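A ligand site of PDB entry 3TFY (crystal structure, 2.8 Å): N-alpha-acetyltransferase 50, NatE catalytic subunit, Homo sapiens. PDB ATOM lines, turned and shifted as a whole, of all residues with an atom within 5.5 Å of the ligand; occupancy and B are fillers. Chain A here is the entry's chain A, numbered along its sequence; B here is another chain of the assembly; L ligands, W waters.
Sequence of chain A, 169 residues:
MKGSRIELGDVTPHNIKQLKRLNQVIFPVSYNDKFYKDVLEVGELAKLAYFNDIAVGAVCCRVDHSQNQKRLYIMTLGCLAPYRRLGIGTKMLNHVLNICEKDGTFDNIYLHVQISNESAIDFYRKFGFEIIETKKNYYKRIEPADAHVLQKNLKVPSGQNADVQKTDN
OD1 of Asn 117 sits close to N of Ala 120 (3.2 Å).
The backbone carbonyl oxygen of Cys 79 is in hydrogen-bond range of the guanidinium group of Arg 84.
O of Tyr 83 is in hydrogen-bond range of SG of Cys 79, 3.6 Å away.
N of Met 1 of chain B lies close to O of Met 75, at 3.5 Å.
The backbone NH (N) of Met 1 of chain B sits at hydrogen-bond distance from the backbone carbonyl oxygen (O) of His 112 (2.6 Å).
Water W2 bridges O4 of the ligand (2.8 Å) and NZ of Lys 126 (2.9 Å).
Water W5 lies within hydrogen-bond range of OG of Ser 119 (2.6 Å), OD1 of Asn 117 (2.7 Å) and N6 of the ligand (2.8 Å).
Water W3 bridges O5 of the ligand (3.0 Å) and N of Gly 87 (3.4 Å).
An oxygen (O9) of the ligand sits at hydrogen-bond distance from the backbone NH (N) of Thr 90, 2.9 Å away.
O9 of the ligand sits at hydrogen-bond distance from OG1 of Thr 90 (2.5 Å).
N of Gly 89 is in hydrogen-bond range of O11 of the ligand (2.6 Å).
N of Arg 85 is in hydrogen-bond range of O12 of the ligand (2.8 Å).
The guanidinium group (NH2) of Arg 85 is in salt-bridge range of an oxygen (O4) of the ligand, at 2.7 Å.
The side-chain amide nitrogen (ND2) of Asn 117 is in hydrogen-bond range of an oxygen (O16) of the ligand (2.7 Å).
The backbone NH of Gly 87 is in hydrogen-bond range of an oxygen (O8) of the ligand.
The backbone NH (N) of Cys 79 sits at hydrogen-bond distance from an oxygen (O15) of the ligand, at 2.9 Å.
The side-chain amino group of Lys 126 sits at hydrogen-bond distance from an oxygen (O1) of the ligand, at 3.0 Å.
N of Met 1 of chain B lies close to S1 of the ligand, 3.1 Å away.
An oxygen (O8) of the ligand sits at hydrogen-bond distance from the backbone NH (N) of Leu 86, 3.2 Å away.
The backbone carbonyl oxygen (O) of Leu 77 lies within hydrogen-bond range of a nitrogen (N7) of the ligand (3.3 Å).
Residues that only touch the ligand: Ile 26 (3.8 Å), Phe 27 (3.5 Å), Gly 78 (3.3 Å), Arg 84 (3.2 Å), Ile 88 (3.6 Å), Leu 111 (3.9 Å), Ser 119 (3.0 Å), Ala 120 (3.8 Å), Asp 122 (3.6 Å), Phe 123 (3.3 Å) and Tyr 124 (3.4 Å).
Hydrophobic or aromatic side chains within 4 Å of the ligand: Ile 26, Phe 27, Ile 88, Leu 111, Ala 120, Phe 123, Tyr 124 and Met 1 of chain B.
The nearest printed residue that does not touch the ligand is Thr 76 (4.3 Å).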
ATOM      1  N   ILE A  26      -5.543 -31.181 -11.298  1.00  0.00           N
ATOM      2  CA  ILE A  26      -4.328 -31.100 -10.503  1.00  0.00           C
ATOM      3  C   ILE A  26      -3.976 -32.429  -9.840  1.00  0.00           C
ATOM      4  O   ILE A  26      -2.818 -32.830  -9.788  1.00  0.00           O
ATOM      5  CB  ILE A  26      -4.463 -30.013  -9.437  1.00  0.00           C
ATOM      6  CG1 ILE A  26      -4.608 -28.646 -10.125  1.00  0.00           C
ATOM      7  CG2 ILE A  26      -3.306 -30.089  -8.425  1.00  0.00           C
ATOM      8  CD1 ILE A  26      -4.789 -27.523  -9.167  1.00  0.00           C
ATOM      9  N   PHE A  27      -4.981 -33.107  -9.329  1.00  0.00           N
ATOM     10  CA  PHE A  27      -4.730 -34.310  -8.559  1.00  0.00           C
ATOM     11  C   PHE A  27      -5.134 -35.585  -9.326  1.00  0.00           C
ATOM     12  O   PHE A  27      -6.175 -35.623  -9.980  1.00  0.00           O
ATOM     13  CB  PHE A  27      -5.425 -34.215  -7.183  1.00  0.00           C
ATOM     14  CG  PHE A  27      -5.020 -32.998  -6.369  1.00  0.00           C
ATOM     15  CD1 PHE A  27      -3.833 -32.988  -5.645  1.00  0.00           C
ATOM     16  CD2 PHE A  27      -5.830 -31.870  -6.321  1.00  0.00           C
ATOM     17  CE1 PHE A  27      -3.469 -31.876  -4.880  1.00  0.00           C
ATOM     18  CE2 PHE A  27      -5.461 -30.768  -5.569  1.00  0.00           C
ATOM     19  CZ  PHE A  27      -4.280 -30.782  -4.845  1.00  0.00           C
ATOM     20  N   ILE A  74      -4.565 -31.636   5.792  1.00  0.00           N
ATOM     21  CA  ILE A  74      -4.655 -31.052   4.467  1.00  0.00           C
ATOM     22  C   ILE A  74      -4.979 -32.143   3.470  1.00  0.00           C
ATOM     23  O   ILE A  74      -4.179 -33.047   3.257  1.00  0.00           O
ATOM     24  CB  ILE A  74      -3.319 -30.407   4.071  1.00  0.00           C
ATOM     25  CG1 ILE A  74      -2.940 -29.268   5.037  1.00  0.00           C
ATOM     26  CG2 ILE A  74      -3.358 -29.904   2.621  1.00  0.00           C
ATOM     27  CD1 ILE A  74      -1.545 -28.611   4.762  1.00  0.00           C
ATOM     28  N   MET A  75      -6.146 -32.072   2.843  1.00  0.00           N
ATOM     29  CA  MET A  75      -6.548 -33.117   1.926  1.00  0.00           C
ATOM     30  C   MET A  75      -6.099 -32.847   0.497  1.00  0.00           C
ATOM     31  O   MET A  75      -5.574 -33.726  -0.182  1.00  0.00           O
ATOM     32  CB  MET A  75      -8.061 -33.296   1.985  1.00  0.00           C
ATOM     33  CG  MET A  75      -8.601 -33.375   3.413  1.00  0.00           C
ATOM     34  SD  MET A  75     -10.391 -33.251   3.423  1.00  0.00           S
ATOM     35  CE  MET A  75     -10.754 -34.838   2.688  1.00  0.00           C
ATOM     36  N   THR A  76      -6.274 -31.615   0.049  1.00  0.00           N
ATOM     37  CA  THR A  76      -5.727 -31.143  -1.202  1.00  0.00           C
ATOM     38  C   THR A  76      -5.204 -29.735  -1.078  1.00  0.00           C
ATOM     39  O   THR A  76      -5.649 -28.993  -0.252  1.00  0.00           O
ATOM     40  CB  THR A  76      -6.741 -31.221  -2.329  1.00  0.00           C
ATOM     41  OG1 THR A  76      -7.562 -30.077  -2.305  1.00  0.00           O
ATOM     42  CG2 THR A  76      -7.585 -32.382  -2.188  1.00  0.00           C
ATOM     43  N   LEU A  77      -4.239 -29.380  -1.896  1.00  0.00           N
ATOM     44  CA  LEU A  77      -3.643 -28.060  -1.936  1.00  0.00           C
ATOM     45  C   LEU A  77      -2.769 -27.961  -3.164  1.00  0.00           C
ATOM     46  O   LEU A  77      -1.691 -28.460  -3.173  1.00  0.00           O
ATOM     47  CB  LEU A  77      -2.801 -27.808  -0.706  1.00  0.00           C
ATOM     48  CG  LEU A  77      -2.400 -26.385  -0.341  1.00  0.00           C
ATOM     49  CD1 LEU A  77      -1.940 -26.312   1.042  1.00  0.00           C
ATOM     50  CD2 LEU A  77      -1.327 -25.943  -1.194  1.00  0.00           C
ATOM     51  N   GLY A  78      -3.230 -27.329  -4.220  1.00  0.00           N
ATOM     52  CA  GLY A  78      -2.462 -27.276  -5.431  1.00  0.00           C
ATOM     53  C   GLY A  78      -2.845 -26.192  -6.397  1.00  0.00           C
ATOM     54  O   GLY A  78      -3.784 -25.502  -6.146  1.00  0.00           O
ATOM     55  N   CYS A  79      -2.110 -26.042  -7.489  1.00  0.00           N
ATOM     56  CA  CYS A  79      -2.437 -25.025  -8.472  1.00  0.00           C
ATOM     57  C   CYS A  79      -1.923 -25.460  -9.837  1.00  0.00           C
ATOM     58  O   CYS A  79      -0.822 -25.993  -9.940  1.00  0.00           O
ATOM     59  CB  CYS A  79      -1.906 -23.654  -8.016  1.00  0.00           C
ATOM     60  SG  CYS A  79      -0.464 -22.900  -8.840  1.00  0.00           S
ATOM     61  N   LEU A  80      -2.731 -25.233 -10.876  1.00  0.00           N
ATOM     62  CA  LEU A  80      -2.362 -25.580 -12.243  1.00  0.00           C
ATOM     63  C   LEU A  80      -0.911 -25.298 -12.630  1.00  0.00           C
ATOM     64  O   LEU A  80      -0.352 -24.231 -12.330  1.00  0.00           O
ATOM     65  CB  LEU A  80      -3.218 -24.825 -13.257  1.00  0.00           C
ATOM     66  CG  LEU A  80      -4.713 -24.786 -12.903  1.00  0.00           C
ATOM     67  CD1 LEU A  80      -5.502 -23.917 -13.865  1.00  0.00           C
ATOM     68  CD2 LEU A  80      -5.286 -26.192 -12.848  1.00  0.00           C
ATOM     69  N   TYR A  83       0.872 -21.975 -13.617  1.00  0.00           N
ATOM     70  CA  TYR A  83       0.918 -20.907 -12.626  1.00  0.00           C
ATOM     71  C   TYR A  83       1.781 -21.220 -11.388  1.00  0.00           C
ATOM     72  O   TYR A  83       1.736 -20.483 -10.403  1.00  0.00           O
ATOM     73  CB  TYR A  83      -0.495 -20.531 -12.182  1.00  0.00           C
ATOM     74  CG  TYR A  83      -1.370 -20.084 -13.329  1.00  0.00           C
ATOM     75  CD1 TYR A  83      -1.364 -18.768 -13.773  1.00  0.00           C
ATOM     76  CD2 TYR A  83      -2.194 -20.982 -13.974  1.00  0.00           C
ATOM     77  CE1 TYR A  83      -2.158 -18.367 -14.822  1.00  0.00           C
ATOM     78  CE2 TYR A  83      -2.994 -20.584 -15.030  1.00  0.00           C
ATOM     79  CZ  TYR A  83      -2.978 -19.282 -15.450  1.00  0.00           C
ATOM     80  OH  TYR A  83      -3.788 -18.920 -16.499  1.00  0.00           O
ATOM     81  N   ARG A  84       2.549 -22.311 -11.444  1.00  0.00           N
ATOM     82  CA  ARG A  84       3.379 -22.677 -10.292  1.00  0.00           C
ATOM     83  C   ARG A  84       4.591 -21.791 -10.125  1.00  0.00           C
ATOM     84  O   ARG A  84       4.972 -21.064 -11.035  1.00  0.00           O
ATOM     85  CB  ARG A  84       3.819 -24.121 -10.404  1.00  0.00           C
ATOM     86  CG  ARG A  84       2.696 -25.055 -10.114  1.00  0.00           C
ATOM     87  CD  ARG A  84       2.978 -26.481 -10.440  1.00  0.00           C
ATOM     88  NE  ARG A  84       1.689 -27.154 -10.459  1.00  0.00           N
ATOM     89  CZ  ARG A  84       1.483 -28.412 -10.809  1.00  0.00           C
ATOM     90  NH1 ARG A  84       2.520 -29.175 -11.171  1.00  0.00           N
ATOM     91  NH2 ARG A  84       0.247 -28.891 -10.782  1.00  0.00           N
ATOM     92  N   ARG A  85       5.205 -21.878  -8.941  1.00  0.00           N
ATOM     93  CA  ARG A  85       6.364 -21.058  -8.620  1.00  0.00           C
ATOM     94  C   ARG A  85       6.054 -19.577  -8.786  1.00  0.00           C
ATOM     95  O   ARG A  85       6.925 -18.800  -9.221  1.00  0.00           O
ATOM     96  CB  ARG A  85       7.560 -21.416  -9.493  1.00  0.00           C
ATOM     97  CG  ARG A  85       8.081 -22.835  -9.325  1.00  0.00           C
ATOM     98  CD  ARG A  85       8.400 -23.188  -7.876  1.00  0.00           C
ATOM     99  NE  ARG A  85       9.683 -22.651  -7.415  1.00  0.00           N
ATOM    100  CZ  ARG A  85      10.855 -23.208  -7.679  1.00  0.00           C
ATOM    101  NH1 ARG A  85      10.922 -24.314  -8.403  1.00  0.00           N
ATOM    102  NH2 ARG A  85      11.965 -22.655  -7.212  1.00  0.00           N
ATOM    103  N   LEU A  86       4.825 -19.172  -8.462  1.00  0.00           N
ATOM    104  CA  LEU A  86       4.499 -17.757  -8.398  1.00  0.00           C
ATOM    105  C   LEU A  86       4.121 -17.335  -6.987  1.00  0.00           C
ATOM    106  O   LEU A  86       3.737 -16.188  -6.757  1.00  0.00           O
ATOM    107  CB  LEU A  86       3.355 -17.416  -9.360  1.00  0.00           C
ATOM    108  CG  LEU A  86       3.610 -17.508 -10.864  1.00  0.00           C
ATOM    109  CD1 LEU A  86       2.341 -17.092 -11.618  1.00  0.00           C
ATOM    110  CD2 LEU A  86       4.810 -16.667 -11.282  1.00  0.00           C
ATOM    111  N   GLY A  87       4.193 -18.262  -6.042  1.00  0.00           N
ATOM    112  CA  GLY A  87       3.867 -17.953  -4.668  1.00  0.00           C
ATOM    113  C   GLY A  87       2.424 -18.191  -4.290  1.00  0.00           C
ATOM    114  O   GLY A  87       1.998 -17.818  -3.189  1.00  0.00           O
ATOM    115  N   ILE A  88       1.665 -18.816  -5.186  1.00  0.00           N
ATOM    116  CA  ILE A  88       0.260 -19.118  -4.942  1.00  0.00           C
ATOM    117  C   ILE A  88       0.054 -20.158  -3.840  1.00  0.00           C
ATOM    118  O   ILE A  88      -0.766 -19.975  -2.936  1.00  0.00           O
ATOM    119  CB  ILE A  88      -0.433 -19.581  -6.232  1.00  0.00           C
ATOM    120  CG1 ILE A  88      -0.674 -18.366  -7.130  1.00  0.00           C
ATOM    121  CG2 ILE A  88      -1.718 -20.324  -5.917  1.00  0.00           C
ATOM    122  CD1 ILE A  88      -1.334 -18.702  -8.437  1.00  0.00           C
ATOM    123  N   GLY A  89       0.806 -21.245  -3.912  1.00  0.00           N
ATOM    124  CA  GLY A  89       0.758 -22.294  -2.912  1.00  0.00           C
ATOM    125  C   GLY A  89       1.114 -21.759  -1.541  1.00  0.00           C
ATOM    126  O   GLY A  89       0.520 -22.177  -0.521  1.00  0.00           O
ATOM    127  N   THR A  90       2.069 -20.838  -1.495  1.00  0.00           N
ATOM    128  CA  THR A  90       2.465 -20.236  -0.231  1.00  0.00           C
ATOM    129  C   THR A  90       1.285 -19.494   0.400  1.00  0.00           C
ATOM    130  O   THR A  90       1.099 -19.526   1.613  1.00  0.00           O
ATOM    131  CB  THR A  90       3.627 -19.269  -0.433  1.00  0.00           C
ATOM    132  OG1 THR A  90       4.711 -19.987  -1.027  1.00  0.00           O
ATOM    133  CG2 THR A  90       4.070 -18.709   0.890  1.00  0.00           C
ATOM    134  N   LYS A  91       0.502 -18.845  -0.448  1.00  0.00           N
ATOM    135  CA  LYS A  91      -0.644 -18.057  -0.002  1.00  0.00           C
ATOM    136  C   LYS A  91      -1.630 -19.008   0.686  1.00  0.00           C
ATOM    137  O   LYS A  91      -2.030 -18.782   1.821  1.00  0.00           O
ATOM    138  CB  LYS A  91      -1.292 -17.345  -1.193  1.00  0.00           C
ATOM    139  CG  LYS A  91      -2.375 -16.323  -0.853  1.00  0.00           C
ATOM    140  CD  LYS A  91      -1.749 -14.987  -0.532  1.00  0.00           C
ATOM    141  CE  LYS A  91      -2.762 -13.874  -0.367  1.00  0.00           C
ATOM    142  NZ  LYS A  91      -2.040 -12.579  -0.453  1.00  0.00           N
ATOM    143  N   LEU A 111      -0.276 -34.263   6.200  1.00  0.00           N
ATOM    144  CA  LEU A 111      -0.829 -34.562   4.890  1.00  0.00           C
ATOM    145  C   LEU A 111      -0.045 -35.696   4.268  1.00  0.00           C
ATOM    146  O   LEU A 111       1.047 -36.021   4.743  1.00  0.00           O
ATOM    147  CB  LEU A 111      -0.735 -33.349   3.978  1.00  0.00           C
ATOM    148  CG  LEU A 111       0.647 -32.945   3.468  1.00  0.00           C
ATOM    149  CD1 LEU A 111       0.528 -32.075   2.228  1.00  0.00           C
ATOM    150  CD2 LEU A 111       1.468 -32.227   4.530  1.00  0.00           C
ATOM    151  N   HIS A 112      -0.599 -36.298   3.211  1.00  0.00           N
ATOM    152  CA  HIS A 112       0.061 -37.400   2.500  1.00  0.00           C
ATOM    153  C   HIS A 112       0.580 -36.961   1.126  1.00  0.00           C
ATOM    154  O   HIS A 112      -0.030 -36.115   0.467  1.00  0.00           O
ATOM    155  CB  HIS A 112      -0.907 -38.577   2.297  1.00  0.00           C
ATOM    156  CG  HIS A 112      -1.179 -39.348   3.544  1.00  0.00           C
ATOM    157  ND1 HIS A 112      -2.266 -39.107   4.353  1.00  0.00           N
ATOM    158  CD2 HIS A 112      -0.492 -40.366   4.131  1.00  0.00           C
ATOM    159  CE1 HIS A 112      -2.248 -39.929   5.377  1.00  0.00           C
ATOM    160  NE2 HIS A 112      -1.185 -40.710   5.262  1.00  0.00           N
ATOM    161  N   VAL A 113       1.688 -37.567   0.706  1.00  0.00           N
ATOM    162  CA  VAL A 113       2.266 -37.292  -0.600  1.00  0.00           C
ATOM    163  C   VAL A 113       2.831 -38.561  -1.271  1.00  0.00           C
ATOM    164  O   VAL A 113       3.548 -39.341  -0.638  1.00  0.00           O
ATOM    165  CB  VAL A 113       3.410 -36.286  -0.478  1.00  0.00           C
ATOM    166  CG1 VAL A 113       4.081 -36.077  -1.804  1.00  0.00           C
ATOM    167  CG2 VAL A 113       2.885 -34.957   0.037  1.00  0.00           C
ATOM    168  N   ASN A 117       6.543 -37.253  -5.614  1.00  0.00           N
ATOM    169  CA  ASN A 117       6.258 -35.830  -5.609  1.00  0.00           C
ATOM    170  C   ASN A 117       7.406 -35.047  -4.994  1.00  0.00           C
ATOM    171  O   ASN A 117       7.332 -34.599  -3.831  1.00  0.00           O
ATOM    172  CB  ASN A 117       4.965 -35.557  -4.815  1.00  0.00           C
ATOM    173  CG  ASN A 117       4.272 -34.278  -5.232  1.00  0.00           C
ATOM    174  OD1 ASN A 117       4.882 -33.349  -5.789  1.00  0.00           O
ATOM    175  ND2 ASN A 117       2.974 -34.212  -4.969  1.00  0.00           N
ATOM    176  N   SER A 119       8.595 -32.065  -5.844  1.00  0.00           N
ATOM    177  CA  SER A 119       8.350 -30.632  -5.678  1.00  0.00           C
ATOM    178  C   SER A 119       7.489 -30.310  -4.430  1.00  0.00           C
ATOM    179  O   SER A 119       7.709 -29.298  -3.742  1.00  0.00           O
ATOM    180  CB  SER A 119       7.795 -29.983  -6.968  1.00  0.00           C
ATOM    181  OG  SER A 119       6.477 -30.408  -7.262  1.00  0.00           O
ATOM    182  N   ALA A 120       6.545 -31.180  -4.128  1.00  0.00           N
ATOM    183  CA  ALA A 120       5.719 -30.979  -2.940  1.00  0.00           C
ATOM    184  C   ALA A 120       6.547 -31.129  -1.645  1.00  0.00           C
ATOM    185  O   ALA A 120       6.286 -30.423  -0.657  1.00  0.00           O
ATOM    186  CB  ALA A 120       4.505 -31.903  -2.962  1.00  0.00           C
ATOM    187  N   ASP A 122       9.938 -30.409  -1.450  1.00  0.00           N
ATOM    188  CA  ASP A 122      10.700 -29.168  -1.377  1.00  0.00           C
ATOM    189  C   ASP A 122       9.837 -28.068  -0.813  1.00  0.00           C
ATOM    190  O   ASP A 122      10.286 -27.250   0.009  1.00  0.00           O
ATOM    191  CB  ASP A 122      11.174 -28.746  -2.764  1.00  0.00           C
ATOM    192  CG  ASP A 122      12.268 -29.636  -3.303  1.00  0.00           C
ATOM    193  OD1 ASP A 122      13.209 -29.920  -2.536  1.00  0.00           O
ATOM    194  OD2 ASP A 122      12.152 -30.057  -4.478  1.00  0.00           O
ATOM    195  N   PHE A 123       8.589 -28.050  -1.269  1.00  0.00           N
ATOM    196  CA  PHE A 123       7.630 -27.040  -0.847  1.00  0.00           C
ATOM    197  C   PHE A 123       7.331 -27.157   0.635  1.00  0.00           C
ATOM    198  O   PHE A 123       7.523 -26.191   1.387  1.00  0.00           O
ATOM    199  CB  PHE A 123       6.347 -27.178  -1.662  1.00  0.00           C
ATOM    200  CG  PHE A 123       5.259 -26.246  -1.245  1.00  0.00           C
ATOM    201  CD1 PHE A 123       5.345 -24.885  -1.532  1.00  0.00           C
ATOM    202  CD2 PHE A 123       4.134 -26.716  -0.591  1.00  0.00           C
ATOM    203  CE1 PHE A 123       4.320 -24.011  -1.168  1.00  0.00           C
ATOM    204  CE2 PHE A 123       3.097 -25.855  -0.213  1.00  0.00           C
ATOM    205  CZ  PHE A 123       3.198 -24.490  -0.512  1.00  0.00           C
ATOM    206  N   TYR A 124       6.879 -28.321   1.070  1.00  0.00           N
ATOM    207  CA  TYR A 124       6.412 -28.435   2.430  1.00  0.00           C
ATOM    208  C   TYR A 124       7.550 -28.391   3.425  1.00  0.00           C
ATOM    209  O   TYR A 124       7.346 -28.021   4.583  1.00  0.00           O
ATOM    210  CB  TYR A 124       5.594 -29.709   2.631  1.00  0.00           C
ATOM    211  CG  TYR A 124       4.153 -29.550   2.228  1.00  0.00           C
ATOM    212  CD1 TYR A 124       3.276 -28.813   3.012  1.00  0.00           C
ATOM    213  CD2 TYR A 124       3.681 -30.114   1.058  1.00  0.00           C
ATOM    214  CE1 TYR A 124       1.937 -28.657   2.651  1.00  0.00           C
ATOM    215  CE2 TYR A 124       2.356 -29.975   0.693  1.00  0.00           C
ATOM    216  CZ  TYR A 124       1.488 -29.245   1.486  1.00  0.00           C
ATOM    217  OH  TYR A 124       0.165 -29.106   1.107  1.00  0.00           O
ATOM    218  N   LYS A 126      10.118 -26.485   3.162  1.00  0.00           N
ATOM    219  CA  LYS A 126      10.494 -25.093   3.311  1.00  0.00           C
ATOM    220  C   LYS A 126       9.756 -24.531   4.510  1.00  0.00           C
ATOM    221  O   LYS A 126      10.277 -23.690   5.219  1.00  0.00           O
ATOM    222  CB  LYS A 126      10.147 -24.295   2.046  1.00  0.00           C
ATOM    223  CG  LYS A 126      11.280 -23.390   1.552  1.00  0.00           C
ATOM    224  CD  LYS A 126      10.729 -22.138   0.818  1.00  0.00           C
ATOM    225  CE  LYS A 126      11.843 -21.158   0.388  1.00  0.00           C
ATOM    226  NZ  LYS A 126      13.029 -21.885  -0.214  1.00  0.00           N
ATOM    227  N   PHE A 127       8.550 -25.031   4.756  1.00  0.00           N
ATOM    228  CA  PHE A 127       7.703 -24.479   5.806  1.00  0.00           C
ATOM    229  C   PHE A 127       7.907 -25.116   7.157  1.00  0.00           C
ATOM    230  O   PHE A 127       7.332 -24.690   8.142  1.00  0.00           O
ATOM    231  CB  PHE A 127       6.230 -24.566   5.399  1.00  0.00           C
ATOM    232  CG  PHE A 127       5.845 -23.556   4.345  1.00  0.00           C
ATOM    233  CD1 PHE A 127       5.128 -22.431   4.662  1.00  0.00           C
ATOM    234  CD2 PHE A 127       6.254 -23.734   3.030  1.00  0.00           C
ATOM    235  CE1 PHE A 127       4.791 -21.513   3.684  1.00  0.00           C
ATOM    236  CE2 PHE A 127       5.926 -22.823   2.060  1.00  0.00           C
ATOM    237  CZ  PHE A 127       5.199 -21.712   2.377  1.00  0.00           C
ATOM    238  N   MET B   1      -2.390 -35.145  -0.212  1.00  0.00           N
ATOM    239  CA  MET B   1      -3.385 -35.723  -1.105  1.00  0.00           C
ATOM    240  C   MET B   1      -3.961 -37.036  -0.564  1.00  0.00           C
ATOM    241  O   MET B   1      -3.330 -38.093  -0.661  1.00  0.00           O
ATOM    242  CB  MET B   1      -2.803 -35.936  -2.510  1.00  0.00           C
ATOM    243  CG  MET B   1      -3.751 -36.653  -3.453  1.00  0.00           C
ATOM    244  SD  MET B   1      -3.113 -36.790  -5.134  1.00  0.00           S
ATOM    245  CE  MET B   1      -1.519 -37.556  -4.831  1.00  0.00           C
HETATM  246  N1  LIG L   1      11.455 -27.256  -6.990  1.00  0.00           N
HETATM  247  C1  LIG L   1      12.124 -26.692  -5.966  1.00  0.00           C
HETATM  248  N2  LIG L   1      11.500 -25.998  -5.004  1.00  0.00           N
HETATM  249  C2  LIG L   1      10.143 -25.845  -5.038  1.00  0.00           C
HETATM  250  C3  LIG L   1       9.427 -26.418  -6.089  1.00  0.00           C
HETATM  251  C4  LIG L   1      10.110 -27.125  -7.065  1.00  0.00           C
HETATM  252  N3  LIG L   1       9.410 -27.668  -8.086  1.00  0.00           N
HETATM  253  N4  LIG L   1       8.125 -26.127  -5.904  1.00  0.00           N
HETATM  254  C5  LIG L   1       8.027 -25.393  -4.775  1.00  0.00           C
HETATM  255  N5  LIG L   1       9.249 -25.232  -4.249  1.00  0.00           N
HETATM  256  C6  LIG L   1       9.562 -24.471  -3.019  1.00  0.00           C
HETATM  257  C7  LIG L   1      10.399 -23.290  -3.447  1.00  0.00           C
HETATM  258  O1  LIG L   1      11.334 -23.005  -2.415  1.00  0.00           O
HETATM  259  C8  LIG L   1       9.362 -22.213  -3.640  1.00  0.00           C
HETATM  260  O2  LIG L   1       9.901 -20.915  -3.500  1.00  0.00           O
HETATM  261  P1  LIG L   1      10.502 -20.218  -4.821  1.00  0.00           P
HETATM  262  O3  LIG L   1      10.753 -18.805  -4.354  1.00  0.00           O
HETATM  263  O4  LIG L   1      11.754 -21.044  -5.073  1.00  0.00           O
HETATM  264  O5  LIG L   1       9.389 -20.321  -5.852  1.00  0.00           O
HETATM  265  C9  LIG L   1       8.397 -22.492  -2.512  1.00  0.00           C
HETATM  266  O6  LIG L   1       8.367 -23.922  -2.450  1.00  0.00           O
HETATM  267  C10 LIG L   1       7.033 -21.863  -2.741  1.00  0.00           C
HETATM  268  O7  LIG L   1       6.529 -22.154  -4.038  1.00  0.00           O
HETATM  269  P2  LIG L   1       5.068 -21.612  -4.475  1.00  0.00           P
HETATM  270  O8  LIG L   1       5.167 -20.865  -5.779  1.00  0.00           O
HETATM  271  O9  LIG L   1       4.379 -20.963  -3.318  1.00  0.00           O
HETATM  272  O10 LIG L   1       4.402 -23.034  -4.774  1.00  0.00           O
HETATM  273  P3  LIG L   1       3.281 -23.341  -5.893  1.00  0.00           P
HETATM  274  O11 LIG L   1       2.213 -22.284  -5.874  1.00  0.00           O
HETATM  275  O12 LIG L   1       3.945 -23.706  -7.199  1.00  0.00           O
HETATM  276  O13 LIG L   1       2.717 -24.674  -5.184  1.00  0.00           O
HETATM  277  C11 LIG L   1       2.606 -27.119  -5.199  1.00  0.00           C
HETATM  278  C12 LIG L   1       3.501 -25.873  -5.110  1.00  0.00           C
HETATM  279  C13 LIG L   1       3.296 -28.270  -4.476  1.00  0.00           C
HETATM  280  C14 LIG L   1       1.270 -26.882  -4.515  1.00  0.00           C
HETATM  281  C15 LIG L   1       2.416 -27.377  -6.715  1.00  0.00           C
HETATM  282  O14 LIG L   1       3.633 -27.778  -7.355  1.00  0.00           O
HETATM  283  C16 LIG L   1       1.331 -28.354  -7.060  1.00  0.00           C
HETATM  284  O15 LIG L   1       0.131 -27.914  -7.407  1.00  0.00           O
HETATM  285  N6  LIG L   1       1.560 -29.662  -7.001  1.00  0.00           N
HETATM  286  C17 LIG L   1       0.590 -30.693  -7.320  1.00  0.00           C
HETATM  287  C18 LIG L   1      -0.338 -30.782  -6.121  1.00  0.00           C
HETATM  288  C19 LIG L   1       0.258 -31.617  -5.014  1.00  0.00           C
HETATM  289  O16 LIG L   1       0.721 -32.735  -5.236  1.00  0.00           O
HETATM  290  N7  LIG L   1       0.219 -31.096  -3.786  1.00  0.00           N
HETATM  291  C20 LIG L   1       0.706 -31.689  -2.544  1.00  0.00           C
HETATM  292  C21 LIG L   1      -0.282 -31.258  -1.463  1.00  0.00           C
HETATM  293  S1  LIG L   1      -1.669 -32.421  -1.464  1.00  0.00           S
HETATM  294  O   HOH W   1       5.787 -25.813  -7.618  1.00  0.00           O
HETATM  295  O   HOH W   2      13.578 -21.382  -2.995  1.00  0.00           O
HETATM  296  O   HOH W   3       7.258 -18.643  -4.623  1.00  0.00           O
HETATM  297  O   HOH W   4       2.602 -20.280  -7.618  1.00  0.00           O
HETATM  298  O   HOH W   5       3.991 -31.140  -7.125  1.00  0.00           O
